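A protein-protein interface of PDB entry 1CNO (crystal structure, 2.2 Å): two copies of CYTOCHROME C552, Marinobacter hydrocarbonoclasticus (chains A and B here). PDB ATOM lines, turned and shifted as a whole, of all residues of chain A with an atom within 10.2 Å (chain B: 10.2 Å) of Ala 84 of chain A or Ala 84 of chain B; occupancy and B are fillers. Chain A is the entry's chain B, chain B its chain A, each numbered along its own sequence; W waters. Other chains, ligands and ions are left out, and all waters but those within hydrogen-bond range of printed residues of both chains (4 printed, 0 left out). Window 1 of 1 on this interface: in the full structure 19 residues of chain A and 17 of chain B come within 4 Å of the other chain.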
ATOM      1  N   HIS A  18      -6.980  12.564   9.125  1.00  0.00           N
ATOM      2  CA  HIS A  18      -6.130  13.658   8.664  1.00  0.00           C
ATOM      3  C   HIS A  18      -5.817  14.735   9.712  1.00  0.00           C
ATOM      4  O   HIS A  18      -5.164  15.723   9.394  1.00  0.00           O
ATOM      5  CB  HIS A  18      -6.732  14.283   7.412  1.00  0.00           C
ATOM      6  CG  HIS A  18      -6.832  13.328   6.249  1.00  0.00           C
ATOM      7  ND1 HIS A  18      -5.717  12.806   5.603  1.00  0.00           N
ATOM      8  CD2 HIS A  18      -7.900  12.785   5.650  1.00  0.00           C
ATOM      9  CE1 HIS A  18      -6.153  11.976   4.642  1.00  0.00           C
ATOM     10  NE2 HIS A  18      -7.466  11.916   4.616  1.00  0.00           N
ATOM     11  N   ASN A  21      -6.443  19.461  12.652  1.00  0.00           N
ATOM     12  CA  ASN A  21      -5.794  20.595  11.999  1.00  0.00           C
ATOM     13  C   ASN A  21      -5.306  20.280  10.575  1.00  0.00           C
ATOM     14  O   ASN A  21      -4.483  21.020  10.023  1.00  0.00           O
ATOM     15  CB  ASN A  21      -4.585  21.036  12.835  1.00  0.00           C
ATOM     16  CG  ASN A  21      -3.514  19.955  12.921  1.00  0.00           C
ATOM     17  OD1 ASN A  21      -3.783  18.765  12.694  1.00  0.00           O
ATOM     18  ND2 ASN A  21      -2.298  20.363  13.266  1.00  0.00           N
ATOM     19  N   GLY A  22      -5.758  19.164  10.005  1.00  0.00           N
ATOM     20  CA  GLY A  22      -5.314  18.812   8.665  1.00  0.00           C
ATOM     21  C   GLY A  22      -3.916  18.205   8.644  1.00  0.00           C
ATOM     22  O   GLY A  22      -3.372  17.931   7.572  1.00  0.00           O
ATOM     23  N   ILE A  23      -3.307  18.070   9.819  1.00  0.00           N
ATOM     24  CA  ILE A  23      -1.992  17.446   9.938  1.00  0.00           C
ATOM     25  C   ILE A  23      -2.265  16.097  10.586  1.00  0.00           C
ATOM     26  O   ILE A  23      -2.821  16.018  11.688  1.00  0.00           O
ATOM     27  CB  ILE A  23      -1.021  18.233  10.863  1.00  0.00           C
ATOM     28  CG1 ILE A  23      -0.740  19.633  10.287  1.00  0.00           C
ATOM     29  CG2 ILE A  23       0.288  17.428  11.066  1.00  0.00           C
ATOM     30  CD1 ILE A  23      -0.194  19.621   8.871  1.00  0.00           C
ATOM     31  N   SER A  24      -1.943  15.036   9.865  1.00  0.00           N
ATOM     32  CA  SER A  24      -2.144  13.685  10.343  1.00  0.00           C
ATOM     33  C   SER A  24      -1.240  13.390  11.549  1.00  0.00           C
ATOM     34  O   SER A  24      -0.210  14.058  11.761  1.00  0.00           O
ATOM     35  CB  SER A  24      -1.813  12.724   9.198  1.00  0.00           C
ATOM     36  OG  SER A  24      -1.934  11.384   9.612  1.00  0.00           O
ATOM     37  N   PRO A  30      -1.969  11.037   4.793  1.00  0.00           N
ATOM     38  CA  PRO A  30      -1.367  12.321   4.404  1.00  0.00           C
ATOM     39  C   PRO A  30      -1.871  13.598   5.117  1.00  0.00           C
ATOM     40  O   PRO A  30      -2.994  13.657   5.632  1.00  0.00           O
ATOM     41  CB  PRO A  30      -1.650  12.382   2.891  1.00  0.00           C
ATOM     42  CG  PRO A  30      -2.959  11.646   2.758  1.00  0.00           C
ATOM     43  CD  PRO A  30      -2.766  10.455   3.691  1.00  0.00           C
ATOM     44  N   ASN A  31      -0.988  14.591   5.205  1.00  0.00           N
ATOM     45  CA  ASN A  31      -1.354  15.898   5.741  1.00  0.00           C
ATOM     46  C   ASN A  31      -2.121  16.537   4.575  1.00  0.00           C
ATOM     47  O   ASN A  31      -1.864  16.220   3.398  1.00  0.00           O
ATOM     48  CB  ASN A  31      -0.114  16.746   6.053  1.00  0.00           C
ATOM     49  CG  ASN A  31       0.733  16.157   7.169  1.00  0.00           C
ATOM     50  OD1 ASN A  31       0.226  15.468   8.042  1.00  0.00           O
ATOM     51  ND2 ASN A  31       2.025  16.425   7.138  1.00  0.00           N
ATOM     52  N   LEU A  32      -3.094  17.385   4.900  1.00  0.00           N
ATOM     53  CA  LEU A  32      -3.907  18.053   3.890  1.00  0.00           C
ATOM     54  C   LEU A  32      -3.831  19.562   4.033  1.00  0.00           C
ATOM     55  O   LEU A  32      -4.084  20.291   3.071  1.00  0.00           O
ATOM     56  CB  LEU A  32      -5.379  17.636   4.024  1.00  0.00           C
ATOM     57  CG  LEU A  32      -5.736  16.149   3.967  1.00  0.00           C
ATOM     58  CD1 LEU A  32      -7.257  16.028   4.029  1.00  0.00           C
ATOM     59  CD2 LEU A  32      -5.176  15.462   2.690  1.00  0.00           C
ATOM     60  N   ALA A  33      -3.543  20.011   5.256  1.00  0.00           N
ATOM     61  CA  ALA A  33      -3.457  21.426   5.601  1.00  0.00           C
ATOM     62  C   ALA A  33      -2.571  22.260   4.683  1.00  0.00           C
ATOM     63  O   ALA A  33      -1.364  22.004   4.540  1.00  0.00           O
ATOM     64  CB  ALA A  33      -3.008  21.598   7.078  1.00  0.00           C
ATOM     65  N   GLY A  34      -3.178  23.279   4.086  1.00  0.00           N
ATOM     66  CA  GLY A  34      -2.437  24.169   3.203  1.00  0.00           C
ATOM     67  C   GLY A  34      -2.047  23.586   1.857  1.00  0.00           C
ATOM     68  O   GLY A  34      -1.217  24.164   1.156  1.00  0.00           O
ATOM     69  N   GLN A  35      -2.597  22.429   1.502  1.00  0.00           N
ATOM     70  CA  GLN A  35      -2.290  21.826   0.205  1.00  0.00           C
ATOM     71  C   GLN A  35      -3.019  22.686  -0.848  1.00  0.00           C
ATOM     72  O   GLN A  35      -3.998  23.374  -0.514  1.00  0.00           O
ATOM     73  CB  GLN A  35      -2.784  20.363   0.164  1.00  0.00           C
ATOM     74  CG  GLN A  35      -2.534  19.620  -1.151  1.00  0.00           C
ATOM     75  CD  GLN A  35      -1.059  19.619  -1.558  1.00  0.00           C
ATOM     76  OE1 GLN A  35      -0.619  20.492  -2.330  1.00  0.00           O
ATOM     77  NE2 GLN A  35      -0.288  18.656  -1.032  1.00  0.00           N
ATOM     78  N   LYS A  36      -2.516  22.689  -2.085  1.00  0.00           N
ATOM     79  CA  LYS A  36      -3.137  23.426  -3.193  1.00  0.00           C
ATOM     80  C   LYS A  36      -4.600  22.992  -3.333  1.00  0.00           C
ATOM     81  O   LYS A  36      -4.906  21.797  -3.528  1.00  0.00           O
ATOM     82  CB  LYS A  36      -2.424  23.127  -4.520  1.00  0.00           C
ATOM     83  CG  LYS A  36      -0.947  23.481  -4.540  1.00  0.00           C
ATOM     84  CD  LYS A  36      -0.740  24.993  -4.595  1.00  0.00           C
ATOM     85  CE  LYS A  36       0.717  25.284  -4.303  1.00  0.00           C
ATOM     86  NZ  LYS A  36       1.040  26.608  -4.749  1.00  0.00           N
ATOM     87  N   TYR A  78     -11.541  24.503   2.538  1.00  0.00           N
ATOM     88  CA  TYR A  78     -11.227  24.450   3.966  1.00  0.00           C
ATOM     89  C   TYR A  78      -9.798  23.968   4.223  1.00  0.00           C
ATOM     90  O   TYR A  78      -9.019  24.662   4.884  1.00  0.00           O
ATOM     91  CB  TYR A  78     -12.216  23.546   4.711  1.00  0.00           C
ATOM     92  CG  TYR A  78     -11.787  23.232   6.129  1.00  0.00           C
ATOM     93  CD1 TYR A  78     -11.718  24.239   7.107  1.00  0.00           C
ATOM     94  CD2 TYR A  78     -11.456  21.927   6.500  1.00  0.00           C
ATOM     95  CE1 TYR A  78     -11.333  23.940   8.419  1.00  0.00           C
ATOM     96  CE2 TYR A  78     -11.064  21.619   7.814  1.00  0.00           C
ATOM     97  CZ  TYR A  78     -11.011  22.633   8.760  1.00  0.00           C
ATOM     98  OH  TYR A  78     -10.651  22.312  10.047  1.00  0.00           O
ATOM     99  N   TYR A  79      -9.427  22.799   3.692  1.00  0.00           N
ATOM    100  CA  TYR A  79      -8.075  22.313   3.953  1.00  0.00           C
ATOM    101  C   TYR A  79      -6.973  23.216   3.383  1.00  0.00           C
ATOM    102  O   TYR A  79      -5.948  23.445   4.041  1.00  0.00           O
ATOM    103  CB  TYR A  79      -7.925  20.839   3.546  1.00  0.00           C
ATOM    104  CG  TYR A  79      -8.551  19.875   4.552  1.00  0.00           C
ATOM    105  CD1 TYR A  79      -8.019  19.737   5.845  1.00  0.00           C
ATOM    106  CD2 TYR A  79      -9.677  19.127   4.222  1.00  0.00           C
ATOM    107  CE1 TYR A  79      -8.594  18.872   6.778  1.00  0.00           C
ATOM    108  CE2 TYR A  79     -10.264  18.256   5.152  1.00  0.00           C
ATOM    109  CZ  TYR A  79      -9.720  18.134   6.425  1.00  0.00           C
ATOM    110  OH  TYR A  79     -10.306  17.275   7.334  1.00  0.00           O
ATOM    111  N   ALA A  80      -7.200  23.780   2.197  1.00  0.00           N
ATOM    112  CA  ALA A  80      -6.213  24.685   1.589  1.00  0.00           C
ATOM    113  C   ALA A  80      -6.008  25.928   2.457  1.00  0.00           C
ATOM    114  O   ALA A  80      -4.892  26.445   2.555  1.00  0.00           O
ATOM    115  CB  ALA A  80      -6.662  25.118   0.178  1.00  0.00           C
ATOM    116  N   SER A  81      -7.085  26.390   3.098  1.00  0.00           N
ATOM    117  CA  SER A  81      -7.041  27.585   3.956  1.00  0.00           C
ATOM    118  C   SER A  81      -6.271  27.396   5.265  1.00  0.00           C
ATOM    119  O   SER A  81      -5.887  28.375   5.884  1.00  0.00           O
ATOM    120  CB  SER A  81      -8.467  28.063   4.300  1.00  0.00           C
ATOM    121  OG  SER A  81      -9.040  27.286   5.351  1.00  0.00           O
ATOM    122  N   ASN A  82      -6.067  26.155   5.703  1.00  0.00           N
ATOM    123  CA  ASN A  82      -5.344  25.898   6.956  1.00  0.00           C
ATOM    124  C   ASN A  82      -3.833  26.075   6.760  1.00  0.00           C
ATOM    125  O   ASN A  82      -3.311  25.817   5.684  1.00  0.00           O
ATOM    126  CB  ASN A  82      -5.598  24.464   7.464  1.00  0.00           C
ATOM    127  CG  ASN A  82      -6.997  24.255   8.052  1.00  0.00           C
ATOM    128  OD1 ASN A  82      -7.608  25.155   8.669  1.00  0.00           O
ATOM    129  ND2 ASN A  82      -7.473  23.021   7.944  1.00  0.00           N
ATOM    130  N   PRO A  83      -3.111  26.521   7.806  1.00  0.00           N
ATOM    131  CA  PRO A  83      -1.657  26.707   7.693  1.00  0.00           C
ATOM    132  C   PRO A  83      -0.977  25.332   7.602  1.00  0.00           C
ATOM    133  O   PRO A  83      -1.280  24.429   8.374  1.00  0.00           O
ATOM    134  CB  PRO A  83      -1.301  27.450   8.991  1.00  0.00           C
ATOM    135  CG  PRO A  83      -2.354  26.984   9.977  1.00  0.00           C
ATOM    136  CD  PRO A  83      -3.614  26.987   9.114  1.00  0.00           C
ATOM    137  N   ALA A  84      -0.070  25.173   6.645  1.00  0.00           N
ATOM    138  CA  ALA A  84       0.624  23.900   6.432  1.00  0.00           C
ATOM    139  C   ALA A  84       1.401  23.372   7.633  1.00  0.00           C
ATOM    140  O   ALA A  84       1.611  22.163   7.754  1.00  0.00           O
ATOM    141  CB  ALA A  84       1.544  24.007   5.234  1.00  0.00           C
ATOM    142  N   ALA A  85       1.816  24.281   8.513  1.00  0.00           N
ATOM    143  CA  ALA A  85       2.588  23.936   9.706  1.00  0.00           C
ATOM    144  C   ALA A  85       1.741  23.791  10.968  1.00  0.00           C
ATOM    145  O   ALA A  85       2.128  23.069  11.889  1.00  0.00           O
ATOM    146  CB  ALA A  85       3.681  24.978   9.932  1.00  0.00           C
ATOM    147  N   ALA A  86       0.605  24.492  10.994  1.00  0.00           N
ATOM    148  CA  ALA A  86      -0.358  24.522  12.109  1.00  0.00           C
ATOM    149  C   ALA A  86      -0.126  25.708  13.051  1.00  0.00           C
ATOM    150  O   ALA A  86      -0.752  25.739  14.133  1.00  0.00           O
ATOM    151  CB  ALA A  86      -0.364  23.200  12.895  1.00  0.00           C
ATOM    152  N   HIS B  18       7.351  20.868  -8.481  1.00  0.00           N
ATOM    153  CA  HIS B  18       7.041  20.873  -7.056  1.00  0.00           C
ATOM    154  C   HIS B  18       7.745  21.966  -6.246  1.00  0.00           C
ATOM    155  O   HIS B  18       7.564  22.051  -5.026  1.00  0.00           O
ATOM    156  CB  HIS B  18       7.310  19.492  -6.464  1.00  0.00           C
ATOM    157  CG  HIS B  18       6.399  18.413  -7.008  1.00  0.00           C
ATOM    158  ND1 HIS B  18       5.030  18.385  -6.724  1.00  0.00           N
ATOM    159  CD2 HIS B  18       6.638  17.397  -7.822  1.00  0.00           C
ATOM    160  CE1 HIS B  18       4.524  17.338  -7.399  1.00  0.00           C
ATOM    161  NE2 HIS B  18       5.453  16.703  -8.082  1.00  0.00           N
ATOM    162  N   ASN B  21      11.653  24.280  -2.813  1.00  0.00           N
ATOM    163  CA  ASN B  21      11.454  24.037  -1.392  1.00  0.00           C
ATOM    164  C   ASN B  21      10.295  23.075  -1.107  1.00  0.00           C
ATOM    165  O   ASN B  21       9.855  22.968   0.035  1.00  0.00           O
ATOM    166  CB  ASN B  21      11.191  25.363  -0.681  1.00  0.00           C
ATOM    167  CG  ASN B  21       9.934  26.036  -1.178  1.00  0.00           C
ATOM    168  OD1 ASN B  21       9.321  25.588  -2.164  1.00  0.00           O
ATOM    169  ND2 ASN B  21       9.539  27.116  -0.516  1.00  0.00           N
ATOM    170  N   GLY B  22       9.789  22.395  -2.135  1.00  0.00           N
ATOM    171  CA  GLY B  22       8.684  21.469  -1.928  1.00  0.00           C
ATOM    172  C   GLY B  22       7.322  22.143  -1.963  1.00  0.00           C
ATOM    173  O   GLY B  22       6.315  21.486  -1.741  1.00  0.00           O
ATOM    174  N   ILE B  23       7.294  23.459  -2.181  1.00  0.00           N
ATOM    175  CA  ILE B  23       6.041  24.212  -2.282  1.00  0.00           C
ATOM    176  C   ILE B  23       5.972  24.617  -3.754  1.00  0.00           C
ATOM    177  O   ILE B  23       6.914  25.235  -4.278  1.00  0.00           O
ATOM    178  CB  ILE B  23       6.042  25.514  -1.441  1.00  0.00           C
ATOM    179  CG1 ILE B  23       6.472  25.240   0.006  1.00  0.00           C
ATOM    180  CG2 ILE B  23       4.653  26.190  -1.498  1.00  0.00           C
ATOM    181  CD1 ILE B  23       5.613  24.224   0.761  1.00  0.00           C
ATOM    182  N   SER B  24       4.888  24.257  -4.434  1.00  0.00           N
ATOM    183  CA  SER B  24       4.770  24.587  -5.855  1.00  0.00           C
ATOM    184  C   SER B  24       4.154  25.967  -6.108  1.00  0.00           C
ATOM    185  O   SER B  24       3.625  26.596  -5.194  1.00  0.00           O
ATOM    186  CB  SER B  24       3.948  23.514  -6.579  1.00  0.00           C
ATOM    187  OG  SER B  24       2.601  23.536  -6.145  1.00  0.00           O
ATOM    188  N   PRO B  30       0.828  19.474  -6.550  1.00  0.00           N
ATOM    189  CA  PRO B  30       0.829  19.448  -5.086  1.00  0.00           C
ATOM    190  C   PRO B  30       2.132  19.814  -4.369  1.00  0.00           C
ATOM    191  O   PRO B  30       3.239  19.656  -4.905  1.00  0.00           O
ATOM    192  CB  PRO B  30       0.420  17.999  -4.767  1.00  0.00           C
ATOM    193  CG  PRO B  30       0.925  17.214  -5.936  1.00  0.00           C
ATOM    194  CD  PRO B  30       0.608  18.125  -7.111  1.00  0.00           C
ATOM    195  N   ASN B  31       1.972  20.367  -3.166  1.00  0.00           N
ATOM    196  CA  ASN B  31       3.103  20.692  -2.297  1.00  0.00           C
ATOM    197  C   ASN B  31       3.545  19.352  -1.714  1.00  0.00           C
ATOM    198  O   ASN B  31       2.698  18.512  -1.398  1.00  0.00           O
ATOM    199  CB  ASN B  31       2.674  21.588  -1.130  1.00  0.00           C
ATOM    200  CG  ASN B  31       2.134  22.928  -1.584  1.00  0.00           C
ATOM    201  OD1 ASN B  31       2.555  23.460  -2.599  1.00  0.00           O
ATOM    202  ND2 ASN B  31       1.202  23.486  -0.816  1.00  0.00           N
ATOM    203  N   LEU B  32       4.860  19.160  -1.587  1.00  0.00           N
ATOM    204  CA  LEU B  32       5.439  17.940  -1.028  1.00  0.00           C
ATOM    205  C   LEU B  32       6.155  18.166   0.315  1.00  0.00           C
ATOM    206  O   LEU B  32       6.307  17.237   1.098  1.00  0.00           O
ATOM    207  CB  LEU B  32       6.433  17.316  -2.018  1.00  0.00           C
ATOM    208  CG  LEU B  32       5.975  16.994  -3.461  1.00  0.00           C
ATOM    209  CD1 LEU B  32       7.093  16.233  -4.211  1.00  0.00           C
ATOM    210  CD2 LEU B  32       4.657  16.173  -3.449  1.00  0.00           C
ATOM    211  N   ALA B  33       6.566  19.399   0.583  1.00  0.00           N
ATOM    212  CA  ALA B  33       7.301  19.732   1.803  1.00  0.00           C
ATOM    213  C   ALA B  33       6.624  19.379   3.128  1.00  0.00           C
ATOM    214  O   ALA B  33       5.509  19.820   3.399  1.00  0.00           O
ATOM    215  CB  ALA B  33       7.709  21.217   1.793  1.00  0.00           C
ATOM    216  N   GLY B  34       7.328  18.588   3.945  1.00  0.00           N
ATOM    217  CA  GLY B  34       6.821  18.195   5.247  1.00  0.00           C
ATOM    218  C   GLY B  34       5.701  17.178   5.230  1.00  0.00           C
ATOM    219  O   GLY B  34       5.063  16.959   6.258  1.00  0.00           O
ATOM    220  N   GLN B  35       5.442  16.576   4.069  1.00  0.00           N
ATOM    221  CA  GLN B  35       4.390  15.569   3.949  1.00  0.00           C
ATOM    222  C   GLN B  35       4.897  14.314   4.681  1.00  0.00           C
ATOM    223  O   GLN B  35       6.102  14.168   4.886  1.00  0.00           O
ATOM    224  CB  GLN B  35       4.137  15.264   2.460  1.00  0.00           C
ATOM    225  CG  GLN B  35       3.042  14.234   2.170  1.00  0.00           C
ATOM    226  CD  GLN B  35       1.750  14.573   2.888  1.00  0.00           C
ATOM    227  OE1 GLN B  35       1.520  14.107   4.015  1.00  0.00           O
ATOM    228  NE2 GLN B  35       0.922  15.422   2.273  1.00  0.00           N
ATOM    229  N   LYS B  36       3.987  13.439   5.102  1.00  0.00           N
ATOM    230  CA  LYS B  36       4.390  12.204   5.777  1.00  0.00           C
ATOM    231  C   LYS B  36       5.254  11.394   4.813  1.00  0.00           C
ATOM    232  O   LYS B  36       4.861  11.145   3.675  1.00  0.00           O
ATOM    233  CB  LYS B  36       3.172  11.370   6.201  1.00  0.00           C
ATOM    234  CG  LYS B  36       2.231  12.073   7.156  1.00  0.00           C
ATOM    235  CD  LYS B  36       2.798  12.189   8.562  1.00  0.00           C
ATOM    236  CE  LYS B  36       1.886  13.093   9.391  1.00  0.00           C
ATOM    237  NZ  LYS B  36       2.221  13.017  10.803  1.00  0.00           N
ATOM    238  N   TYR B  78      13.772  13.149   1.800  1.00  0.00           N
ATOM    239  CA  TYR B  78      14.117  14.538   1.541  1.00  0.00           C
ATOM    240  C   TYR B  78      12.926  15.477   1.690  1.00  0.00           C
ATOM    241  O   TYR B  78      12.983  16.429   2.472  1.00  0.00           O
ATOM    242  CB  TYR B  78      14.725  14.682   0.140  1.00  0.00           C
ATOM    243  CG  TYR B  78      14.892  16.119  -0.305  1.00  0.00           C
ATOM    244  CD1 TYR B  78      15.700  17.010   0.414  1.00  0.00           C
ATOM    245  CD2 TYR B  78      14.209  16.601  -1.418  1.00  0.00           C
ATOM    246  CE1 TYR B  78      15.831  18.347   0.021  1.00  0.00           C
ATOM    247  CE2 TYR B  78      14.336  17.927  -1.818  1.00  0.00           C
ATOM    248  CZ  TYR B  78      15.141  18.798  -1.091  1.00  0.00           C
ATOM    249  OH  TYR B  78      15.248  20.112  -1.505  1.00  0.00           O
ATOM    250  N   TYR B  79      11.857  15.219   0.932  1.00  0.00           N
ATOM    251  CA  TYR B  79      10.661  16.063   0.987  1.00  0.00           C
ATOM    252  C   TYR B  79      10.015  16.101   2.361  1.00  0.00           C
ATOM    253  O   TYR B  79       9.628  17.167   2.826  1.00  0.00           O
ATOM    254  CB  TYR B  79       9.663  15.666  -0.100  1.00  0.00           C
ATOM    255  CG  TYR B  79      10.064  16.173  -1.464  1.00  0.00           C
ATOM    256  CD1 TYR B  79      10.117  17.544  -1.711  1.00  0.00           C
ATOM    257  CD2 TYR B  79      10.417  15.294  -2.503  1.00  0.00           C
ATOM    258  CE1 TYR B  79      10.518  18.042  -2.937  1.00  0.00           C
ATOM    259  CE2 TYR B  79      10.830  15.795  -3.764  1.00  0.00           C
ATOM    260  CZ  TYR B  79      10.870  17.172  -3.957  1.00  0.00           C
ATOM    261  OH  TYR B  79      11.274  17.715  -5.140  1.00  0.00           O
ATOM    262  N   ALA B  80       9.953  14.953   3.031  1.00  0.00           N
ATOM    263  CA  ALA B  80       9.375  14.880   4.373  1.00  0.00           C
ATOM    264  C   ALA B  80      10.159  15.754   5.374  1.00  0.00           C
ATOM    265  O   ALA B  80       9.564  16.349   6.287  1.00  0.00           O
ATOM    266  CB  ALA B  80       9.348  13.444   4.856  1.00  0.00           C
ATOM    267  N   SER B  81      11.470  15.883   5.154  1.00  0.00           N
ATOM    268  CA  SER B  81      12.353  16.658   6.047  1.00  0.00           C
ATOM    269  C   SER B  81      12.249  18.169   5.877  1.00  0.00           C
ATOM    270  O   SER B  81      12.682  18.924   6.746  1.00  0.00           O
ATOM    271  CB  SER B  81      13.817  16.231   5.872  1.00  0.00           C
ATOM    272  OG  SER B  81      14.364  16.792   4.690  1.00  0.00           O
ATOM    273  N   ASN B  82      11.699  18.607   4.750  1.00  0.00           N
ATOM    274  CA  ASN B  82      11.536  20.030   4.461  1.00  0.00           C
ATOM    275  C   ASN B  82      10.409  20.629   5.311  1.00  0.00           C
ATOM    276  O   ASN B  82       9.455  19.940   5.670  1.00  0.00           O
ATOM    277  CB  ASN B  82      11.179  20.226   2.981  1.00  0.00           C
ATOM    278  CG  ASN B  82      12.401  20.262   2.054  1.00  0.00           C
ATOM    279  OD1 ASN B  82      13.555  20.373   2.499  1.00  0.00           O
ATOM    280  ND2 ASN B  82      12.138  20.243   0.744  1.00  0.00           N
ATOM    281  N   PRO B  83      10.532  21.908   5.692  1.00  0.00           N
ATOM    282  CA  PRO B  83       9.494  22.568   6.495  1.00  0.00           C
ATOM    283  C   PRO B  83       8.254  22.816   5.625  1.00  0.00           C
ATOM    284  O   PRO B  83       8.356  23.375   4.523  1.00  0.00           O
ATOM    285  CB  PRO B  83      10.167  23.879   6.917  1.00  0.00           C
ATOM    286  CG  PRO B  83      11.127  24.113   5.835  1.00  0.00           C
ATOM    287  CD  PRO B  83      11.712  22.777   5.554  1.00  0.00           C
ATOM    288  N   ALA B  84       7.096  22.407   6.133  1.00  0.00           N
ATOM    289  CA  ALA B  84       5.825  22.542   5.416  1.00  0.00           C
ATOM    290  C   ALA B  84       5.487  23.965   4.986  1.00  0.00           C
ATOM    291  O   ALA B  84       4.727  24.170   4.036  1.00  0.00           O
ATOM    292  CB  ALA B  84       4.687  21.964   6.267  1.00  0.00           C
ATOM    293  N   ALA B  85       6.067  24.944   5.681  1.00  0.00           N
ATOM    294  CA  ALA B  85       5.844  26.365   5.412  1.00  0.00           C
ATOM    295  C   ALA B  85       6.862  27.029   4.469  1.00  0.00           C
ATOM    296  O   ALA B  85       6.538  28.046   3.847  1.00  0.00           O
ATOM    297  CB  ALA B  85       5.764  27.136   6.739  1.00  0.00           C
ATOM    298  N   ALA B  86       8.080  26.476   4.428  1.00  0.00           N
ATOM    299  CA  ALA B  86       9.213  26.903   3.590  1.00  0.00           C
ATOM    300  C   ALA B  86      10.484  27.315   4.331  1.00  0.00           C
ATOM    301  O   ALA B  86      10.738  28.510   4.477  1.00  0.00           O
ATOM    302  CB  ALA B  86       8.829  27.983   2.613  1.00  0.00           C
HETATM  303  O   HOH W   1       3.950  15.676   9.324  1.00  0.00           O
HETATM  304  O   HOH W   2       0.852  21.802   1.810  1.00  0.00           O
HETATM  305  O   HOH W   3       0.350  26.309  -1.394  1.00  0.00           O
HETATM  306  O   HOH W   4       1.804  16.006  -0.509  1.00  0.00           O
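The backbone carbonyl oxygen (O) of Ser 24 of chain B is in hydrogen-bond range of the side-chain amino group (NZ) of Lys 36 of chain A. ND2 of Asn 31 of chain B sits at hydrogen-bond distance from O of Gly 34 of chain A, at 3.2 Å. The backbone NH (N) of Asn 31 of chain B is in hydrogen-bond range of the side-chain amide oxygen (OE1) of Gln 35 of chain A (2.7 Å). The backbone carbonyl oxygen (O) of Gly 34 of chain B sits at hydrogen-bond distance from the side-chain amide nitrogen (ND2) of Asn 31 of chain A (3.2 Å). The backbone NH (N) of Asn 31 of chain A is in hydrogen-bond range of the side-chain amide oxygen (OE1) of Gln 35 of chain B, at 2.8 Å. NZ of Lys 36 of chain B sits at hydrogen-bond distance from O of Ser 24 of chain A (2.8 Å).
A ring nitrogen (ND1) of His 18 of chain B is in hydrogen-bond range of the backbone carbonyl oxygen (O) of Pro 30 of chain B, 2.9 Å away. N of Ser 24 of chain B is in hydrogen-bond range of OD1 of Asn 31 of chain B, 3.1 Å away. The backbone carbonyl oxygen (O) of Pro 30 of chain A is in hydrogen-bond range of a ring nitrogen (ND1) of His 18 of chain A (2.9 Å).
Among the printed residues, merely in contact across the chains: Lys 36 of chain A with Asn 31 of chain B (3.1 Å), Asn 31 of chain A with Lys 36 of chain B (3.2 Å), Gln 35 of chain A with Pro 30 of chain B (3.3 Å), Ala 84 of chain A with Ala 84 of chain B (3.4 Å) and Pro 30 of chain A with Gln 35 of chain B (3.4 Å).
Ala 84 of chain A touches just one residue of chain B: Ala 84 (3.4 Å). Ala 84 of chain B touches just one residue of chain A: Ala 84. No residue of chain B comes within 4 Å of Ala 33 of chain A. Gly 34 of chain A touches one residue of chain B. No residue of chain A comes within 4 Å of Ala 85 of chain B. Printed residues of chain B within 4 Å of Asn 31 of chain A: Gly 34, Gln 35 and Lys 36. Of the printed residues of chain A, Lys 36 of chain B touches Ser 24 (2.8 Å) and Asn 31 (3.2 Å). His 18 of chain A touches none of the printed residues of chain B. His 18 of chain B touches none of the printed residues of chain A. The nearest residue of chain A that does not touch Ala 84 of chain B is Ala 85 of chain A (4.3 Å). The nearest printed residue of chain A that does not touch Pro 30 of chain B is Lys 36 of chain A (4.4 Å).
Among the printed residues, no Asp or Glu carboxylate lies within 4 Å of a Lys or Arg side-chain nitrogen of the other chain.
Ser 24 of chain A touches Lys 36 of chain B, and with the chains exchanged Lys 36 of chain A touches Ser 24 of chain B. Asn 31 of chain A touches Gln 35 of chain B, and with the chains exchanged Gln 35 of chain A touches Asn 31 of chain B. Asn 31 of chain A touches Lys 36 of chain B, and with the chains exchanged Lys 36 of chain A touches Asn 31 of chain B. Ala 84 of chain B touches its own counterpart, Ala 84 of chain A.
Water W4 lies within hydrogen-bond range of the backbone carbonyl oxygen of Asn 31 of chain B (2.8 Å), the side-chain amide nitrogen of Gln 35 of chain B (3.0 Å) and the side-chain amide nitrogen of Gln 35 of chain A (3.4 Å). Water W3 bridges ND2 of Asn 31 of chain B and NZ of Lys 36 of chain A. Water W1 bridges ND2 of Asn 31 of chain A and NZ of Lys 36 of chain B.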
